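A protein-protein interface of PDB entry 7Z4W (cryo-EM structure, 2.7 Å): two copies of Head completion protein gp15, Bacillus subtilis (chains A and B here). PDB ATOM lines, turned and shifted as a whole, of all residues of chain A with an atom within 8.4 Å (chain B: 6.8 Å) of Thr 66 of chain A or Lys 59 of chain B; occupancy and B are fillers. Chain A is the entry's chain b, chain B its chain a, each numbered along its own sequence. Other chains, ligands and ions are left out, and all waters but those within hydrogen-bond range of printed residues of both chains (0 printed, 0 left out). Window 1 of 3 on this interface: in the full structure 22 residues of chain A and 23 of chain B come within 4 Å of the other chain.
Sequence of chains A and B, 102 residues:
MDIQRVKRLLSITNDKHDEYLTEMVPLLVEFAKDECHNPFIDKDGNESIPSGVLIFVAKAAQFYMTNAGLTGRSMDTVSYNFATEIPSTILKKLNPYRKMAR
The side-chain hydroxyl of Tyr 20 of chain A sits at hydrogen-bond distance from the backbone carbonyl oxygen of Ala 61 of chain A (2.9 Å).
The side-chain amide oxygen (OD1) of Asn 67 of chain A sits close to the backbone NH (N) of Gly 69 of chain A (3.3 Å).
The backbone carbonyl oxygen (O) of Phe 63 of chain A is in hydrogen-bond range of the side-chain hydroxyl (OG1) of Thr 66 of chain A.
The side-chain hydroxyl (OH) of Tyr 20 of chain A lies close to the backbone carbonyl oxygen (O) of Tyr 64 of chain A (3.4 Å).
The side-chain amino group (NZ) of Lys 59 of chain B sits at hydrogen-bond distance from the side-chain amide oxygen (OE1) of Gln 62 of chain B (3.3 Å).
Positions printed for both chains: 60, 61, 62, 63 and 64.
Tyr 20 of chain A touches Leu 9 of chain B (CD1 to O, 3.6 Å).
Met 24 of chain A touches Leu 9 of chain B (CE to CD2, 3.9 Å).
O of Thr 66 of chain A touches NZ of Lys 59 of chain B, at 3.5 Å.
Thr 66 of chain A touches Gln 62 of chain B (O to OE1, 3.6 Å).
Asn 67 of chain A touches Gln 62 of chain B.
Ala 68 of chain A touches Lys 59 of chain B.
Phe 63 of chain B touches Ala 68 of chain A.
CA of Gly 69 of chain A touches CD1 of Phe 63 of chain B, at 3.8 Å.
Of the 17 printed residues of chain B, 4 touch a printed residue of chain A.
Printed residues of chain B that touch a printed residue of chain A: Leu 9, Lys 59, Gln 62 and Phe 63.
Hydrophobic or aromatic side chains of chain B within 4 Å of the printed part of chain A: Leu 9 and Phe 63.
Hydrophobic or aromatic side chains of chain A that line the printed part of chain B: Tyr 20, Met 24, Tyr 64 and Ala 68.
Among the printed residues, no Asp or Glu carboxylate lies within 4 Å of a Lys or Arg side-chain nitrogen of the other chain.
Of chain B, only Lys 59 and Gln 62 come within 4 Å of Thr 66 of chain A.
Of the printed residues of chain B, Met 24 of chain A touches Leu 9.
Printed residues of chain B within 4 Å of Ala 68 of chain A: Lys 59, Gln 62 and Phe 63.
Of the printed residues of chain A, Gln 62 of chain B touches Thr 66, Asn 67 and Ala 68.
Leu 54 of chain B touches none of the printed residues of chain A.
The nearest residue of chain B that does not touch Thr 66 of chain A is Leu 10 of chain B (6.6 Å).
The nearest residue of chain A that does not touch Lys 59 of chain B is Met 65 of chain A (5.3 Å).
The backbone NH of Ala 68 of chain A lies within hydrogen-bond range of the side-chain amide oxygen of Gln 62 of chain B (2.8 Å).
NZ of Lys 59 of chain B lies within hydrogen-bond range of O of Tyr 64 of chain A, 3.3 Å away.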
ATOM      1  N   TYR A  20      -3.056  32.572 -11.236  1.00  0.00           N
ATOM      2  CA  TYR A  20      -4.438  32.301 -10.847  1.00  0.00           C
ATOM      3  C   TYR A  20      -5.417  32.700 -11.948  1.00  0.00           C
ATOM      4  O   TYR A  20      -6.379  31.972 -12.220  1.00  0.00           O
ATOM      5  CB  TYR A  20      -4.767  33.033  -9.541  1.00  0.00           C
ATOM      6  CG  TYR A  20      -6.250  33.206  -9.267  1.00  0.00           C
ATOM      7  CD1 TYR A  20      -7.019  32.145  -8.808  1.00  0.00           C
ATOM      8  CD2 TYR A  20      -6.879  34.433  -9.461  1.00  0.00           C
ATOM      9  CE1 TYR A  20      -8.370  32.296  -8.559  1.00  0.00           C
ATOM     10  CE2 TYR A  20      -8.228  34.588  -9.224  1.00  0.00           C
ATOM     11  CZ  TYR A  20      -8.966  33.519  -8.767  1.00  0.00           C
ATOM     12  OH  TYR A  20     -10.306  33.673  -8.522  1.00  0.00           O
ATOM     13  N   MET A  24      -8.285  30.606 -13.977  1.00  0.00           N
ATOM     14  CA  MET A  24      -9.652  30.833 -13.518  1.00  0.00           C
ATOM     15  C   MET A  24     -10.562  31.460 -14.578  1.00  0.00           C
ATOM     16  O   MET A  24     -11.754  31.141 -14.615  1.00  0.00           O
ATOM     17  CB  MET A  24      -9.622  31.696 -12.247  1.00  0.00           C
ATOM     18  CG  MET A  24     -10.974  32.012 -11.607  1.00  0.00           C
ATOM     19  SD  MET A  24     -12.059  30.587 -11.369  1.00  0.00           S
ATOM     20  CE  MET A  24     -11.773  30.198  -9.649  1.00  0.00           C
ATOM     21  N   ALA A  60     -16.385  37.974 -10.697  1.00  0.00           N
ATOM     22  CA  ALA A  60     -16.371  36.680 -10.025  1.00  0.00           C
ATOM     23  C   ALA A  60     -14.950  36.170  -9.814  1.00  0.00           C
ATOM     24  O   ALA A  60     -14.667  35.535  -8.788  1.00  0.00           O
ATOM     25  CB  ALA A  60     -17.194  35.666 -10.818  1.00  0.00           C
ATOM     26  N   ALA A  61     -14.042  36.454 -10.753  1.00  0.00           N
ATOM     27  CA  ALA A  61     -12.641  36.113 -10.543  1.00  0.00           C
ATOM     28  C   ALA A  61     -12.025  36.939  -9.422  1.00  0.00           C
ATOM     29  O   ALA A  61     -11.158  36.439  -8.699  1.00  0.00           O
ATOM     30  CB  ALA A  61     -11.848  36.295 -11.836  1.00  0.00           C
ATOM     31  N   GLN A  62     -12.460  38.193  -9.254  1.00  0.00           N
ATOM     32  CA  GLN A  62     -11.989  38.963  -8.105  1.00  0.00           C
ATOM     33  C   GLN A  62     -12.576  38.436  -6.798  1.00  0.00           C
ATOM     34  O   GLN A  62     -11.899  38.449  -5.764  1.00  0.00           O
ATOM     35  CB  GLN A  62     -12.313  40.445  -8.277  1.00  0.00           C
ATOM     36  CG  GLN A  62     -11.579  41.340  -7.290  1.00  0.00           C
ATOM     37  CD  GLN A  62     -11.969  42.795  -7.399  1.00  0.00           C
ATOM     38  OE1 GLN A  62     -13.137  43.146  -7.272  1.00  0.00           O
ATOM     39  NE2 GLN A  62     -10.987  43.652  -7.626  1.00  0.00           N
ATOM     40  N   PHE A  63     -13.830  37.972  -6.827  1.00  0.00           N
ATOM     41  CA  PHE A  63     -14.457  37.424  -5.624  1.00  0.00           C
ATOM     42  C   PHE A  63     -13.774  36.141  -5.164  1.00  0.00           C
ATOM     43  O   PHE A  63     -13.607  35.923  -3.960  1.00  0.00           O
ATOM     44  CB  PHE A  63     -15.947  37.168  -5.866  1.00  0.00           C
ATOM     45  CG  PHE A  63     -16.678  36.622  -4.662  1.00  0.00           C
ATOM     46  CD1 PHE A  63     -17.153  37.477  -3.683  1.00  0.00           C
ATOM     47  CD2 PHE A  63     -16.896  35.255  -4.512  1.00  0.00           C
ATOM     48  CE1 PHE A  63     -17.821  36.983  -2.576  1.00  0.00           C
ATOM     49  CE2 PHE A  63     -17.559  34.761  -3.407  1.00  0.00           C
ATOM     50  CZ  PHE A  63     -18.021  35.625  -2.440  1.00  0.00           C
ATOM     51  N   TYR A  64     -13.389  35.273  -6.097  1.00  0.00           N
ATOM     52  CA  TYR A  64     -12.858  33.968  -5.712  1.00  0.00           C
ATOM     53  C   TYR A  64     -11.376  33.987  -5.331  1.00  0.00           C
ATOM     54  O   TYR A  64     -10.778  32.917  -5.209  1.00  0.00           O
ATOM     55  CB  TYR A  64     -13.107  32.954  -6.829  1.00  0.00           C
ATOM     56  CG  TYR A  64     -14.503  32.385  -6.787  1.00  0.00           C
ATOM     57  CD1 TYR A  64     -15.029  31.891  -5.602  1.00  0.00           C
ATOM     58  CD2 TYR A  64     -15.304  32.364  -7.920  1.00  0.00           C
ATOM     59  CE1 TYR A  64     -16.307  31.379  -5.546  1.00  0.00           C
ATOM     60  CE2 TYR A  64     -16.588  31.853  -7.876  1.00  0.00           C
ATOM     61  CZ  TYR A  64     -17.081  31.360  -6.686  1.00  0.00           C
ATOM     62  OH  TYR A  64     -18.354  30.851  -6.629  1.00  0.00           O
ATOM     63  N   MET A  65     -10.771  35.158  -5.133  1.00  0.00           N
ATOM     64  CA  MET A  65      -9.437  35.243  -4.555  1.00  0.00           C
ATOM     65  C   MET A  65      -9.435  35.078  -3.041  1.00  0.00           C
ATOM     66  O   MET A  65      -8.358  34.944  -2.453  1.00  0.00           O
ATOM     67  CB  MET A  65      -8.781  36.579  -4.908  1.00  0.00           C
ATOM     68  CG  MET A  65      -8.412  36.753  -6.360  1.00  0.00           C
ATOM     69  SD  MET A  65      -7.633  38.351  -6.664  1.00  0.00           S
ATOM     70  CE  MET A  65      -7.593  38.384  -8.449  1.00  0.00           C
ATOM     71  N   THR A  66     -10.600  35.086  -2.399  1.00  0.00           N
ATOM     72  CA  THR A  66     -10.688  34.939  -0.955  1.00  0.00           C
ATOM     73  C   THR A  66     -10.613  33.467  -0.550  1.00  0.00           C
ATOM     74  O   THR A  66     -10.673  32.558  -1.379  1.00  0.00           O
ATOM     75  CB  THR A  66     -11.982  35.559  -0.427  1.00  0.00           C
ATOM     76  OG1 THR A  66     -13.107  34.936  -1.053  1.00  0.00           O
ATOM     77  CG2 THR A  66     -12.019  37.045  -0.707  1.00  0.00           C
ATOM     78  N   ASN A  67     -10.467  33.244   0.752  1.00  0.00           N
ATOM     79  CA  ASN A  67     -10.519  31.911   1.335  1.00  0.00           C
ATOM     80  C   ASN A  67     -11.969  31.545   1.632  1.00  0.00           C
ATOM     81  O   ASN A  67     -12.694  32.324   2.255  1.00  0.00           O
ATOM     82  CB  ASN A  67      -9.680  31.853   2.611  1.00  0.00           C
ATOM     83  CG  ASN A  67      -9.247  30.451   2.960  1.00  0.00           C
ATOM     84  OD1 ASN A  67     -10.035  29.653   3.458  1.00  0.00           O
ATOM     85  ND2 ASN A  67      -7.985  30.145   2.710  1.00  0.00           N
ATOM     86  N   ALA A  68     -12.381  30.355   1.193  1.00  0.00           N
ATOM     87  CA  ALA A  68     -13.786  29.968   1.264  1.00  0.00           C
ATOM     88  C   ALA A  68     -14.242  29.624   2.676  1.00  0.00           C
ATOM     89  O   ALA A  68     -15.442  29.708   2.959  1.00  0.00           O
ATOM     90  CB  ALA A  68     -14.049  28.785   0.334  1.00  0.00           C
ATOM     91  N   GLY A  69     -13.332  29.241   3.566  1.00  0.00           N
ATOM     92  CA  GLY A  69     -13.727  28.890   4.915  1.00  0.00           C
ATOM     93  C   GLY A  69     -13.522  29.976   5.955  1.00  0.00           C
ATOM     94  O   GLY A  69     -13.474  29.681   7.150  1.00  0.00           O
ATOM     95  N   LEU A  70     -13.429  31.233   5.528  1.00  0.00           N
ATOM     96  CA  LEU A  70     -13.081  32.329   6.424  1.00  0.00           C
ATOM     97  C   LEU A  70     -14.029  33.498   6.210  1.00  0.00           C
ATOM     98  O   LEU A  70     -14.241  33.921   5.072  1.00  0.00           O
ATOM     99  CB  LEU A  70     -11.633  32.773   6.187  1.00  0.00           C
ATOM    100  CG  LEU A  70     -10.821  33.297   7.367  1.00  0.00           C
ATOM    101  CD1 LEU A  70     -10.599  32.204   8.390  1.00  0.00           C
ATOM    102  CD2 LEU A  70      -9.492  33.847   6.879  1.00  0.00           C
ATOM    103  N   THR A  71     -14.599  34.018   7.300  1.00  0.00           N
ATOM    104  CA  THR A  71     -15.415  35.224   7.236  1.00  0.00           C
ATOM    105  C   THR A  71     -14.746  36.456   7.831  1.00  0.00           C
ATOM    106  O   THR A  71     -15.198  37.570   7.557  1.00  0.00           O
ATOM    107  CB  THR A  71     -16.768  35.009   7.938  1.00  0.00           C
ATOM    108  OG1 THR A  71     -16.570  34.794   9.338  1.00  0.00           O
ATOM    109  CG2 THR A  71     -17.496  33.816   7.349  1.00  0.00           C
ATOM    110  N   ASN A  81     -13.026  41.825   7.033  1.00  0.00           N
ATOM    111  CA  ASN A  81     -14.315  41.147   7.015  1.00  0.00           C
ATOM    112  C   ASN A  81     -14.647  40.802   5.572  1.00  0.00           C
ATOM    113  O   ASN A  81     -14.648  41.680   4.708  1.00  0.00           O
ATOM    114  CB  ASN A  81     -15.417  42.021   7.614  1.00  0.00           C
ATOM    115  CG  ASN A  81     -15.257  42.217   9.100  1.00  0.00           C
ATOM    116  OD1 ASN A  81     -15.467  41.296   9.885  1.00  0.00           O
ATOM    117  ND2 ASN A  81     -14.884  43.422   9.498  1.00  0.00           N
ATOM    118  N   PHE A  82     -14.926  39.530   5.315  1.00  0.00           N
ATOM    119  CA  PHE A  82     -15.119  39.037   3.960  1.00  0.00           C
ATOM    120  C   PHE A  82     -16.594  38.800   3.666  1.00  0.00           C
ATOM    121  O   PHE A  82     -17.390  38.511   4.561  1.00  0.00           O
ATOM    122  CB  PHE A  82     -14.332  37.744   3.736  1.00  0.00           C
ATOM    123  CG  PHE A  82     -12.861  37.874   4.004  1.00  0.00           C
ATOM    124  CD1 PHE A  82     -12.054  38.618   3.159  1.00  0.00           C
ATOM    125  CD2 PHE A  82     -12.284  37.251   5.098  1.00  0.00           C
ATOM    126  CE1 PHE A  82     -10.698  38.738   3.401  1.00  0.00           C
ATOM    127  CE2 PHE A  82     -10.930  37.369   5.346  1.00  0.00           C
ATOM    128  CZ  PHE A  82     -10.138  38.112   4.496  1.00  0.00           C
ATOM    129  N   ALA A  83     -16.950  38.931   2.390  1.00  0.00           N
ATOM    130  CA  ALA A  83     -18.287  38.587   1.927  1.00  0.00           C
ATOM    131  C   ALA A  83     -18.392  37.086   1.702  1.00  0.00           C
ATOM    132  O   ALA A  83     -17.467  36.457   1.182  1.00  0.00           O
ATOM    133  CB  ALA A  83     -18.615  39.336   0.637  1.00  0.00           C
ATOM    134  N   THR A  84     -19.524  36.508   2.098  1.00  0.00           N
ATOM    135  CA  THR A  84     -19.674  35.060   2.025  1.00  0.00           C
ATOM    136  C   THR A  84     -20.370  34.586   0.751  1.00  0.00           C
ATOM    137  O   THR A  84     -20.160  33.444   0.337  1.00  0.00           O
ATOM    138  CB  THR A  84     -20.411  34.540   3.268  1.00  0.00           C
ATOM    139  OG1 THR A  84     -20.400  33.108   3.274  1.00  0.00           O
ATOM    140  CG2 THR A  84     -21.849  35.052   3.344  1.00  0.00           C
ATOM    141  N   GLU A  85     -21.175  35.428   0.112  1.00  0.00           N
ATOM    142  CA  GLU A  85     -21.838  35.089  -1.135  1.00  0.00           C
ATOM    143  C   GLU A  85     -21.476  36.106  -2.203  1.00  0.00           C
ATOM    144  O   GLU A  85     -21.111  37.245  -1.905  1.00  0.00           O
ATOM    145  CB  GLU A  85     -23.363  35.043  -0.979  1.00  0.00           C
ATOM    146  CG  GLU A  85     -23.852  34.309   0.238  1.00  0.00           C
ATOM    147  CD  GLU A  85     -23.918  32.815   0.024  1.00  0.00           C
ATOM    148  OE1 GLU A  85     -23.890  32.378  -1.141  1.00  0.00           O
ATOM    149  OE2 GLU A  85     -23.988  32.078   1.025  1.00  0.00           O
ATOM    150  N   VAL B   6      -5.460  22.281  -9.178  1.00  0.00           N
ATOM    151  CA  VAL B   6      -6.185  22.771  -8.006  1.00  0.00           C
ATOM    152  C   VAL B   6      -5.315  23.727  -7.195  1.00  0.00           C
ATOM    153  O   VAL B   6      -5.795  24.758  -6.700  1.00  0.00           O
ATOM    154  CB  VAL B   6      -6.675  21.582  -7.153  1.00  0.00           C
ATOM    155  CG1 VAL B   6      -7.378  22.052  -5.889  1.00  0.00           C
ATOM    156  CG2 VAL B   6      -7.594  20.693  -7.955  1.00  0.00           C
ATOM    157  N   LEU B   9      -5.413  26.936  -8.870  1.00  0.00           N
ATOM    158  CA  LEU B   9      -6.697  27.603  -8.675  1.00  0.00           C
ATOM    159  C   LEU B   9      -6.879  28.155  -7.265  1.00  0.00           C
ATOM    160  O   LEU B   9      -7.711  29.045  -7.072  1.00  0.00           O
ATOM    161  CB  LEU B   9      -7.850  26.649  -8.992  1.00  0.00           C
ATOM    162  CG  LEU B   9      -8.263  26.478 -10.453  1.00  0.00           C
ATOM    163  CD1 LEU B   9      -9.080  25.216 -10.622  1.00  0.00           C
ATOM    164  CD2 LEU B   9      -9.040  27.683 -10.947  1.00  0.00           C
ATOM    165  N   LEU B  10      -6.137  27.657  -6.278  1.00  0.00           N
ATOM    166  CA  LEU B  10      -6.272  28.131  -4.905  1.00  0.00           C
ATOM    167  C   LEU B  10      -5.107  28.992  -4.433  1.00  0.00           C
ATOM    168  O   LEU B  10      -5.086  29.367  -3.255  1.00  0.00           O
ATOM    169  CB  LEU B  10      -6.453  26.950  -3.943  1.00  0.00           C
ATOM    170  CG  LEU B  10      -7.671  26.041  -4.136  1.00  0.00           C
ATOM    171  CD1 LEU B  10      -7.681  24.942  -3.095  1.00  0.00           C
ATOM    172  CD2 LEU B  10      -8.970  26.832  -4.093  1.00  0.00           C
ATOM    173  N   LEU B  28     -14.305  14.178  -3.829  1.00  0.00           N
ATOM    174  CA  LEU B  28     -15.235  15.233  -4.213  1.00  0.00           C
ATOM    175  C   LEU B  28     -15.698  15.078  -5.655  1.00  0.00           C
ATOM    176  O   LEU B  28     -16.843  15.430  -5.972  1.00  0.00           O
ATOM    177  CB  LEU B  28     -14.598  16.605  -3.997  1.00  0.00           C
ATOM    178  CG  LEU B  28     -14.449  17.025  -2.534  1.00  0.00           C
ATOM    179  CD1 LEU B  28     -13.609  18.284  -2.402  1.00  0.00           C
ATOM    180  CD2 LEU B  28     -15.805  17.209  -1.875  1.00  0.00           C
ATOM    181  N   LEU B  54     -15.402  21.530 -11.693  1.00  0.00           N
ATOM    182  CA  LEU B  54     -14.018  21.807 -11.311  1.00  0.00           C
ATOM    183  C   LEU B  54     -13.929  22.964 -10.316  1.00  0.00           C
ATOM    184  O   LEU B  54     -13.177  22.888  -9.328  1.00  0.00           O
ATOM    185  CB  LEU B  54     -13.179  22.100 -12.558  1.00  0.00           C
ATOM    186  CG  LEU B  54     -13.136  21.043 -13.670  1.00  0.00           C
ATOM    187  CD1 LEU B  54     -12.706  21.639 -14.999  1.00  0.00           C
ATOM    188  CD2 LEU B  54     -12.252  19.866 -13.313  1.00  0.00           C
ATOM    189  N   ILE B  55     -14.714  24.025 -10.548  1.00  0.00           N
ATOM    190  CA  ILE B  55     -14.788  25.140  -9.602  1.00  0.00           C
ATOM    191  C   ILE B  55     -15.336  24.675  -8.253  1.00  0.00           C
ATOM    192  O   ILE B  55     -14.812  25.046  -7.189  1.00  0.00           O
ATOM    193  CB  ILE B  55     -15.630  26.285 -10.197  1.00  0.00           C
ATOM    194  CG1 ILE B  55     -14.949  26.860 -11.438  1.00  0.00           C
ATOM    195  CG2 ILE B  55     -15.860  27.393  -9.184  1.00  0.00           C
ATOM    196  CD1 ILE B  55     -15.771  27.896 -12.167  1.00  0.00           C
ATOM    197  N   PHE B  56     -16.365  23.818  -8.282  1.00  0.00           N
ATOM    198  CA  PHE B  56     -16.954  23.297  -7.053  1.00  0.00           C
ATOM    199  C   PHE B  56     -15.970  22.440  -6.265  1.00  0.00           C
ATOM    200  O   PHE B  56     -15.905  22.543  -5.036  1.00  0.00           O
ATOM    201  CB  PHE B  56     -18.210  22.485  -7.373  1.00  0.00           C
ATOM    202  CG  PHE B  56     -18.723  21.717  -6.203  1.00  0.00           C
ATOM    203  CD1 PHE B  56     -19.382  22.379  -5.187  1.00  0.00           C
ATOM    204  CD2 PHE B  56     -18.527  20.345  -6.100  1.00  0.00           C
ATOM    205  CE1 PHE B  56     -19.839  21.704  -4.096  1.00  0.00           C
ATOM    206  CE2 PHE B  56     -18.975  19.668  -5.000  1.00  0.00           C
ATOM    207  CZ  PHE B  56     -19.635  20.354  -3.998  1.00  0.00           C
ATOM    208  N   VAL B  57     -15.211  21.583  -6.955  1.00  0.00           N
ATOM    209  CA  VAL B  57     -14.277  20.685  -6.283  1.00  0.00           C
ATOM    210  C   VAL B  57     -13.140  21.473  -5.641  1.00  0.00           C
ATOM    211  O   VAL B  57     -12.784  21.226  -4.479  1.00  0.00           O
ATOM    212  CB  VAL B  57     -13.769  19.613  -7.270  1.00  0.00           C
ATOM    213  CG1 VAL B  57     -12.526  18.907  -6.749  1.00  0.00           C
ATOM    214  CG2 VAL B  57     -14.853  18.587  -7.529  1.00  0.00           C
ATOM    215  N   ALA B  58     -12.612  22.481  -6.350  1.00  0.00           N
ATOM    216  CA  ALA B  58     -11.547  23.310  -5.781  1.00  0.00           C
ATOM    217  C   ALA B  58     -12.026  24.115  -4.571  1.00  0.00           C
ATOM    218  O   ALA B  58     -11.348  24.145  -3.533  1.00  0.00           O
ATOM    219  CB  ALA B  58     -10.977  24.238  -6.850  1.00  0.00           C
ATOM    220  N   LYS B  59     -13.217  24.719  -4.656  1.00  0.00           N
ATOM    221  CA  LYS B  59     -13.675  25.544  -3.541  1.00  0.00           C
ATOM    222  C   LYS B  59     -14.129  24.711  -2.346  1.00  0.00           C
ATOM    223  O   LYS B  59     -13.938  25.131  -1.200  1.00  0.00           O
ATOM    224  CB  LYS B  59     -14.788  26.485  -3.997  1.00  0.00           C
ATOM    225  CG  LYS B  59     -14.338  27.572  -4.963  1.00  0.00           C
ATOM    226  CD  LYS B  59     -12.993  28.178  -4.583  1.00  0.00           C
ATOM    227  CE  LYS B  59     -13.144  29.403  -3.710  1.00  0.00           C
ATOM    228  NZ  LYS B  59     -11.895  30.207  -3.672  1.00  0.00           N
ATOM    229  N   ALA B  60     -14.692  23.520  -2.578  1.00  0.00           N
ATOM    230  CA  ALA B  60     -15.064  22.657  -1.463  1.00  0.00           C
ATOM    231  C   ALA B  60     -13.841  22.056  -0.782  1.00  0.00           C
ATOM    232  O   ALA B  60     -13.835  21.899   0.447  1.00  0.00           O
ATOM    233  CB  ALA B  60     -16.006  21.554  -1.941  1.00  0.00           C
ATOM    234  N   ALA B  61     -12.794  21.733  -1.553  1.00  0.00           N
ATOM    235  CA  ALA B  61     -11.544  21.293  -0.946  1.00  0.00           C
ATOM    236  C   ALA B  61     -10.888  22.405  -0.138  1.00  0.00           C
ATOM    237  O   ALA B  61     -10.255  22.125   0.885  1.00  0.00           O
ATOM    238  CB  ALA B  61     -10.585  20.780  -2.018  1.00  0.00           C
ATOM    239  N   GLN B  62     -11.031  23.664  -0.566  1.00  0.00           N
ATOM    240  CA  GLN B  62     -10.531  24.760   0.262  1.00  0.00           C
ATOM    241  C   GLN B  62     -11.365  24.940   1.528  1.00  0.00           C
ATOM    242  O   GLN B  62     -10.814  25.234   2.595  1.00  0.00           O
ATOM    243  CB  GLN B  62     -10.485  26.064  -0.532  1.00  0.00           C
ATOM    244  CG  GLN B  62      -9.663  27.149   0.146  1.00  0.00           C
ATOM    245  CD  GLN B  62      -9.723  28.475  -0.572  1.00  0.00           C
ATOM    246  OE1 GLN B  62     -10.795  29.036  -0.773  1.00  0.00           O
ATOM    247  NE2 GLN B  62      -8.565  28.990  -0.954  1.00  0.00           N
ATOM    248  N   PHE B  63     -12.690  24.771   1.430  1.00  0.00           N
ATOM    249  CA  PHE B  63     -13.554  24.928   2.601  1.00  0.00           C
ATOM    250  C   PHE B  63     -13.299  23.849   3.649  1.00  0.00           C
ATOM    251  O   PHE B  63     -13.364  24.124   4.851  1.00  0.00           O
ATOM    252  CB  PHE B  63     -15.031  24.914   2.186  1.00  0.00           C
ATOM    253  CG  PHE B  63     -15.996  25.062   3.340  1.00  0.00           C
ATOM    254  CD1 PHE B  63     -16.329  26.316   3.818  1.00  0.00           C
ATOM    255  CD2 PHE B  63     -16.579  23.948   3.941  1.00  0.00           C
ATOM    256  CE1 PHE B  63     -17.212  26.459   4.875  1.00  0.00           C
ATOM    257  CE2 PHE B  63     -17.452  24.089   4.998  1.00  0.00           C
ATOM    258  CZ  PHE B  63     -17.768  25.345   5.465  1.00  0.00           C
ATOM    259  N   TYR B  64     -13.028  22.618   3.224  1.00  0.00           N
ATOM    260  CA  TYR B  64     -12.888  21.529   4.187  1.00  0.00           C
ATOM    261  C   TYR B  64     -11.506  21.460   4.843  1.00  0.00           C
ATOM    262  O   TYR B  64     -11.213  20.470   5.512  1.00  0.00           O
ATOM    263  CB  TYR B  64     -13.227  20.194   3.523  1.00  0.00           C
ATOM    264  CG  TYR B  64     -14.711  19.936   3.463  1.00  0.00           C
ATOM    265  CD1 TYR B  64     -15.503  20.096   4.590  1.00  0.00           C
ATOM    266  CD2 TYR B  64     -15.327  19.559   2.275  1.00  0.00           C
ATOM    267  CE1 TYR B  64     -16.861  19.876   4.546  1.00  0.00           C
ATOM    268  CE2 TYR B  64     -16.689  19.337   2.218  1.00  0.00           C
ATOM    269  CZ  TYR B  64     -17.449  19.497   3.358  1.00  0.00           C
ATOM    270  OH  TYR B  64     -18.803  19.277   3.312  1.00  0.00           O
ATOM    271  N   ILE B  86     -21.056  25.535   3.680  1.00  0.00           N
ATOM    272  CA  ILE B  86     -20.648  25.878   2.313  1.00  0.00           C
ATOM    273  C   ILE B  86     -21.639  26.891   1.751  1.00  0.00           C
ATOM    274  O   ILE B  86     -22.861  26.687   1.878  1.00  0.00           O
ATOM    275  CB  ILE B  86     -20.586  24.613   1.435  1.00  0.00           C
ATOM    276  CG1 ILE B  86     -19.495  23.673   1.939  1.00  0.00           C
ATOM    277  CG2 ILE B  86     -20.330  24.961  -0.026  1.00  0.00           C
ATOM    278  CD1 ILE B  86     -19.288  22.436   1.091  1.00  0.00           C
ATOM    279  N   ILE B  90     -21.458  28.456  -4.154  1.00  0.00           N
ATOM    280  CA  ILE B  90     -20.588  27.344  -4.525  1.00  0.00           C
ATOM    281  C   ILE B  90     -21.410  26.090  -4.806  1.00  0.00           C
ATOM    282  O   ILE B  90     -21.126  25.348  -5.754  1.00  0.00           O
ATOM    283  CB  ILE B  90     -19.531  27.118  -3.427  1.00  0.00           C
ATOM    284  CG1 ILE B  90     -18.621  28.341  -3.317  1.00  0.00           C
ATOM    285  CG2 ILE B  90     -18.691  25.874  -3.698  1.00  0.00           C
ATOM    286  CD1 ILE B  90     -17.590  28.248  -2.223  1.00  0.00           C
